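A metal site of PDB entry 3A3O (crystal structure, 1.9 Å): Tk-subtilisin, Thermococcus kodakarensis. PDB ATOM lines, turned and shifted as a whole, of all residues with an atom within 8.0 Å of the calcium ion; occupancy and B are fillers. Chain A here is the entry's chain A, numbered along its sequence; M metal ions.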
ATOM      1  N   GLN A  12      -8.029 -22.078  -0.751  1.00  0.00           N
ATOM      2  CA  GLN A  12      -8.577 -22.560   0.575  1.00  0.00           C
ATOM      3  C   GLN A  12      -7.448 -22.799   1.576  1.00  0.00           C
ATOM      4  O   GLN A  12      -6.503 -23.520   1.268  1.00  0.00           O
ATOM      5  CB  GLN A  12      -9.395 -23.847   0.408  1.00  0.00           C
ATOM      6  CG  GLN A  12     -10.774 -23.663  -0.234  1.00  0.00           C
ATOM      7  CD  GLN A  12     -11.739 -22.866   0.647  1.00  0.00           C
ATOM      8  OE1 GLN A  12     -11.752 -23.009   1.869  1.00  0.00           O
ATOM      9  NE2 GLN A  12     -12.527 -21.994   0.034  1.00  0.00           N
ATOM     10  N   PRO A  13      -7.559 -22.226   2.795  1.00  0.00           N
ATOM     11  CA  PRO A  13      -6.535 -22.481   3.808  1.00  0.00           C
ATOM     12  C   PRO A  13      -6.590 -23.895   4.376  1.00  0.00           C
ATOM     13  O   PRO A  13      -7.659 -24.538   4.323  1.00  0.00           O
ATOM     14  CB  PRO A  13      -6.859 -21.465   4.912  1.00  0.00           C
ATOM     15  CG  PRO A  13      -8.357 -21.174   4.741  1.00  0.00           C
ATOM     16  CD  PRO A  13      -8.648 -21.341   3.261  1.00  0.00           C
ATOM     17  N   ALA A  14      -5.454 -24.372   4.922  1.00  0.00           N
ATOM     18  CA  ALA A  14      -5.372 -25.646   5.647  1.00  0.00           C
ATOM     19  C   ALA A  14      -6.275 -25.617   6.876  1.00  0.00           C
ATOM     20  O   ALA A  14      -6.442 -24.551   7.502  1.00  0.00           O
ATOM     21  CB  ALA A  14      -3.929 -25.942   6.052  1.00  0.00           C
ATOM     22  N   GLN A  15      -6.844 -26.777   7.212  1.00  0.00           N
ATOM     23  CA  GLN A  15      -7.823 -26.878   8.312  1.00  0.00           C
ATOM     24  C   GLN A  15      -7.230 -26.550   9.682  1.00  0.00           C
ATOM     25  O   GLN A  15      -6.139 -27.018  10.028  1.00  0.00           O
ATOM     26  CB  GLN A  15      -8.468 -28.268   8.356  1.00  0.00           C
ATOM     27  CG  GLN A  15      -9.573 -28.425   9.413  1.00  0.00           C
ATOM     28  CD  GLN A  15     -10.362 -29.688   9.264  1.00  0.00           C
ATOM     29  OE1 GLN A  15     -11.248 -29.767   8.412  1.00  0.00           O
ATOM     30  NE2 GLN A  15     -10.039 -30.698  10.075  1.00  0.00           N
ATOM     31  N   THR A  16      -7.947 -25.713  10.455  1.00  0.00           N
ATOM     32  CA  THR A  16      -7.692 -25.604  11.896  1.00  0.00           C
ATOM     33  C   THR A  16      -8.913 -26.018  12.652  1.00  0.00           C
ATOM     34  O   THR A  16     -10.022 -25.935  12.123  1.00  0.00           O
ATOM     35  CB  THR A  16      -7.602 -24.161  12.420  1.00  0.00           C
ATOM     36  OG1 THR A  16      -7.866 -23.205  11.378  1.00  0.00           O
ATOM     37  CG2 THR A  16      -6.342 -23.920  13.224  1.00  0.00           C
ATOM     38  N   HIS A  53     -20.248 -23.592  -0.408  1.00  0.00           N
ATOM     39  CA  HIS A  53     -18.984 -23.467   0.310  1.00  0.00           C
ATOM     40  C   HIS A  53     -18.288 -24.826   0.371  1.00  0.00           C
ATOM     41  O   HIS A  53     -18.903 -25.827   0.736  1.00  0.00           O
ATOM     42  CB  HIS A  53     -19.211 -22.901   1.715  1.00  0.00           C
ATOM     43  CG  HIS A  53     -17.943 -22.511   2.410  1.00  0.00           C
ATOM     44  ND1 HIS A  53     -17.715 -21.238   2.868  1.00  0.00           N
ATOM     45  CD2 HIS A  53     -16.839 -23.226   2.710  1.00  0.00           C
ATOM     46  CE1 HIS A  53     -16.530 -21.184   3.453  1.00  0.00           C
ATOM     47  NE2 HIS A  53     -15.965 -22.375   3.353  1.00  0.00           N
ATOM     48  N   PRO A  54     -17.007 -24.911  -0.041  1.00  0.00           N
ATOM     49  CA  PRO A  54     -16.316 -26.226  -0.036  1.00  0.00           C
ATOM     50  C   PRO A  54     -16.238 -26.881   1.343  1.00  0.00           C
ATOM     51  O   PRO A  54     -16.096 -28.116   1.458  1.00  0.00           O
ATOM     52  CB  PRO A  54     -14.891 -25.892  -0.521  1.00  0.00           C
ATOM     53  CG  PRO A  54     -15.029 -24.615  -1.283  1.00  0.00           C
ATOM     54  CD  PRO A  54     -16.151 -23.832  -0.592  1.00  0.00           C
ATOM     55  N   ASP A  55     -16.320 -26.083   2.403  1.00  0.00           N
ATOM     56  CA  ASP A  55     -16.265 -26.663   3.760  1.00  0.00           C
ATOM     57  C   ASP A  55     -17.636 -26.928   4.382  1.00  0.00           C
ATOM     58  O   ASP A  55     -17.716 -27.295   5.565  1.00  0.00           O
ATOM     59  CB  ASP A  55     -15.390 -25.833   4.716  1.00  0.00           C
ATOM     60  CG  ASP A  55     -14.532 -26.727   5.611  1.00  0.00           C
ATOM     61  OD1 ASP A  55     -14.256 -27.892   5.240  1.00  0.00           O
ATOM     62  OD2 ASP A  55     -14.090 -26.299   6.693  1.00  0.00           O
ATOM     63  N   LEU A  56     -18.696 -26.745   3.571  1.00  0.00           N
ATOM     64  CA  LEU A  56     -20.084 -26.956   4.009  1.00  0.00           C
ATOM     65  C   LEU A  56     -20.917 -27.844   3.099  1.00  0.00           C
ATOM     66  O   LEU A  56     -21.858 -28.526   3.553  1.00  0.00           O
ATOM     67  CB  LEU A  56     -20.813 -25.613   4.127  1.00  0.00           C
ATOM     68  CG  LEU A  56     -20.384 -24.557   5.163  1.00  0.00           C
ATOM     69  CD1 LEU A  56     -21.397 -23.442   5.108  1.00  0.00           C
ATOM     70  CD2 LEU A  56     -20.319 -25.131   6.564  1.00  0.00           C
ATOM     71  N   ALA A  93     -21.288 -27.718  11.680  1.00  0.00           N
ATOM     72  CA  ALA A  93     -21.178 -28.802  10.674  1.00  0.00           C
ATOM     73  C   ALA A  93     -20.116 -28.616   9.603  1.00  0.00           C
ATOM     74  O   ALA A  93     -20.153 -29.328   8.568  1.00  0.00           O
ATOM     75  CB  ALA A  93     -22.522 -29.013  10.021  1.00  0.00           C
ATOM     76  N   ALA A  94     -19.165 -27.692   9.827  1.00  0.00           N
ATOM     77  CA  ALA A  94     -18.045 -27.590   8.860  1.00  0.00           C
ATOM     78  C   ALA A  94     -17.348 -28.963   8.755  1.00  0.00           C
ATOM     79  O   ALA A  94     -17.165 -29.652   9.759  1.00  0.00           O
ATOM     80  CB  ALA A  94     -17.061 -26.514   9.272  1.00  0.00           C
ATOM     81  N   LEU A  95     -16.973 -29.362   7.540  1.00  0.00           N
ATOM     82  CA  LEU A  95     -16.478 -30.719   7.293  1.00  0.00           C
ATOM     83  C   LEU A  95     -15.080 -30.942   7.870  1.00  0.00           C
ATOM     84  O   LEU A  95     -14.239 -30.019   7.885  1.00  0.00           O
ATOM     85  CB  LEU A  95     -16.480 -30.961   5.774  1.00  0.00           C
ATOM     86  CG  LEU A  95     -17.874 -31.005   5.140  1.00  0.00           C
ATOM     87  CD1 LEU A  95     -17.878 -30.506   3.666  1.00  0.00           C
ATOM     88  CD2 LEU A  95     -18.452 -32.415   5.225  1.00  0.00           C
ATOM     89  N   ASN A  96     -14.839 -32.159   8.345  1.00  0.00           N
ATOM     90  CA  ASN A  96     -13.522 -32.554   8.835  1.00  0.00           C
ATOM     91  C   ASN A  96     -12.725 -33.075   7.631  1.00  0.00           C
ATOM     92  O   ASN A  96     -12.968 -34.180   7.151  1.00  0.00           O
ATOM     93  CB  ASN A  96     -13.657 -33.638   9.883  1.00  0.00           C
ATOM     94  CG  ASN A  96     -12.342 -33.947  10.586  1.00  0.00           C
ATOM     95  OD1 ASN A  96     -11.326 -33.307  10.312  1.00  0.00           O
ATOM     96  ND2 ASN A  96     -12.360 -34.915  11.485  1.00  0.00           N
ATOM     97  N   ASN A  97     -11.811 -32.251   7.131  1.00  0.00           N
ATOM     98  CA  ASN A  97     -11.106 -32.539   5.879  1.00  0.00           C
ATOM     99  C   ASN A  97      -9.766 -31.801   5.889  1.00  0.00           C
ATOM    100  O   ASN A  97      -9.227 -31.521   6.955  1.00  0.00           O
ATOM    101  CB  ASN A  97     -11.998 -32.149   4.657  1.00  0.00           C
ATOM    102  CG  ASN A  97     -12.496 -30.684   4.699  1.00  0.00           C
ATOM    103  OD1 ASN A  97     -12.001 -29.855   5.474  1.00  0.00           O
ATOM    104  ND2 ASN A  97     -13.457 -30.354   3.825  1.00  0.00           N
ATOM    105  N   ASP A  98      -9.275 -31.416   4.718  1.00  0.00           N
ATOM    106  CA  ASP A  98      -7.980 -30.764   4.648  1.00  0.00           C
ATOM    107  C   ASP A  98      -8.018 -29.247   4.662  1.00  0.00           C
ATOM    108  O   ASP A  98      -6.974 -28.613   4.594  1.00  0.00           O
ATOM    109  CB  ASP A  98      -7.191 -31.283   3.421  1.00  0.00           C
ATOM    110  CG  ASP A  98      -6.967 -32.784   3.469  1.00  0.00           C
ATOM    111  OD1 ASP A  98      -6.532 -33.305   4.536  1.00  0.00           O
ATOM    112  OD2 ASP A  98      -7.225 -33.469   2.442  1.00  0.00           O
ATOM    113  N   ILE A  99      -9.212 -28.667   4.760  1.00  0.00           N
ATOM    114  CA  ILE A  99      -9.390 -27.224   4.593  1.00  0.00           C
ATOM    115  C   ILE A  99     -10.228 -26.538   5.683  1.00  0.00           C
ATOM    116  O   ILE A  99     -11.064 -27.168   6.320  1.00  0.00           O
ATOM    117  CB  ILE A  99     -10.035 -26.880   3.215  1.00  0.00           C
ATOM    118  CG1 ILE A  99     -11.379 -27.624   3.037  1.00  0.00           C
ATOM    119  CG2 ILE A  99      -9.061 -27.240   2.043  1.00  0.00           C
ATOM    120  CD1 ILE A  99     -12.280 -27.003   1.988  1.00  0.00           C
ATOM    121  N   GLY A 100      -9.995 -25.251   5.880  1.00  0.00           N
ATOM    122  CA  GLY A 100     -10.954 -24.391   6.551  1.00  0.00           C
ATOM    123  C   GLY A 100     -11.055 -24.640   8.035  1.00  0.00           C
ATOM    124  O   GLY A 100     -10.072 -24.477   8.764  1.00  0.00           O
ATOM    125  N   VAL A 101     -12.243 -24.988   8.516  1.00  0.00           N
ATOM    126  CA  VAL A 101     -12.437 -25.213   9.950  1.00  0.00           C
ATOM    127  C   VAL A 101     -13.089 -26.588  10.127  1.00  0.00           C
ATOM    128  O   VAL A 101     -13.037 -27.409   9.206  1.00  0.00           O
ATOM    129  CB  VAL A 101     -13.244 -24.050  10.597  1.00  0.00           C
ATOM    130  CG1 VAL A 101     -12.414 -22.751  10.631  1.00  0.00           C
ATOM    131  CG2 VAL A 101     -14.620 -23.823   9.871  1.00  0.00           C
ATOM    132  N   VAL A 102     -13.685 -26.874  11.284  1.00  0.00           N
ATOM    133  CA  VAL A 102     -14.404 -28.129  11.488  1.00  0.00           C
ATOM    134  C   VAL A 102     -15.490 -27.850  12.528  1.00  0.00           C
ATOM    135  O   VAL A 102     -15.240 -27.128  13.478  1.00  0.00           O
ATOM    136  CB  VAL A 102     -13.461 -29.297  11.921  1.00  0.00           C
ATOM    137  CG1 VAL A 102     -12.731 -29.009  13.260  1.00  0.00           C
ATOM    138  CG2 VAL A 102     -14.186 -30.637  11.940  1.00  0.00           C
ATOM    139  N   GLY A 103     -16.682 -28.428  12.322  1.00  0.00           N
ATOM    140  CA  GLY A 103     -17.823 -28.181  13.223  1.00  0.00           C
ATOM    141  C   GLY A 103     -17.770 -29.120  14.411  1.00  0.00           C
ATOM    142  O   GLY A 103     -16.954 -30.048  14.462  1.00  0.00           O
ATOM    143  N   PRO A 106     -19.169 -32.656  12.561  1.00  0.00           N
ATOM    144  CA  PRO A 106     -18.747 -32.424  11.201  1.00  0.00           C
ATOM    145  C   PRO A 106     -19.348 -33.347  10.120  1.00  0.00           C
ATOM    146  O   PRO A 106     -19.078 -33.108   8.945  1.00  0.00           O
ATOM    147  CB  PRO A 106     -17.218 -32.534  11.278  1.00  0.00           C
ATOM    148  CG  PRO A 106     -16.907 -33.334  12.439  1.00  0.00           C
ATOM    149  CD  PRO A 106     -18.075 -33.162  13.409  1.00  0.00           C
ATOM    150  N   THR A 242     -16.954 -20.586   8.902  1.00  0.00           N
ATOM    151  CA  THR A 242     -17.209 -20.322   7.493  1.00  0.00           C
ATOM    152  C   THR A 242     -17.933 -18.965   7.300  1.00  0.00           C
ATOM    153  O   THR A 242     -18.683 -18.504   8.176  1.00  0.00           O
ATOM    154  CB  THR A 242     -18.011 -21.489   6.867  1.00  0.00           C
ATOM    155  OG1 THR A 242     -19.086 -21.837   7.755  1.00  0.00           O
ATOM    156  CG2 THR A 242     -17.087 -22.745   6.727  1.00  0.00           C
ATOM    157  N   TYR A 248     -13.856 -17.381   5.361  1.00  0.00           N
ATOM    158  CA  TYR A 248     -13.898 -17.633   6.819  1.00  0.00           C
ATOM    159  C   TYR A 248     -13.899 -16.274   7.498  1.00  0.00           C
ATOM    160  O   TYR A 248     -13.411 -15.286   6.920  1.00  0.00           O
ATOM    161  CB  TYR A 248     -12.716 -18.550   7.287  1.00  0.00           C
ATOM    162  CG  TYR A 248     -12.702 -19.825   6.514  1.00  0.00           C
ATOM    163  CD1 TYR A 248     -12.060 -19.885   5.263  1.00  0.00           C
ATOM    164  CD2 TYR A 248     -13.443 -20.932   6.933  1.00  0.00           C
ATOM    165  CE1 TYR A 248     -12.119 -21.002   4.482  1.00  0.00           C
ATOM    166  CE2 TYR A 248     -13.502 -22.071   6.163  1.00  0.00           C
ATOM    167  CZ  TYR A 248     -12.836 -22.099   4.928  1.00  0.00           C
ATOM    168  OH  TYR A 248     -12.903 -23.222   4.144  1.00  0.00           O
HETATM  169 CA    CA M   1     -12.808 -28.421   7.158  1.00  0.00          CA
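The calcium ion is bound by the backbone carbonyl oxygen (O) of Leu 95, the backbone carbonyl oxygen (O) of Val 101, the backbone carbonyl oxygen (O) of Ile 99, the side-chain amide oxygen (OD1) of Asn 97, the side-chain amide oxygen (OE1) of Gln 15, the side-chain carboxylate (OD1) of Asp 55 and the side-chain carboxylate (OD2) of Asp 55.
The calcium ion has seven donor atoms within binding distance.
Of the 23 residues printed, 6 come within 4 Å of the calcium ion.
The nearest printed residue that does not touch the calcium ion is Gly 100 (4.3 Å).
The backbone NH of Gln 15 lies within hydrogen-bond range of the backbone carbonyl oxygen of Asp 98.
The side-chain amide nitrogen (NE2) of Gln 15 lies within hydrogen-bond range of the side-chain amide oxygen (OD1) of Asn 96 (2.9 Å).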
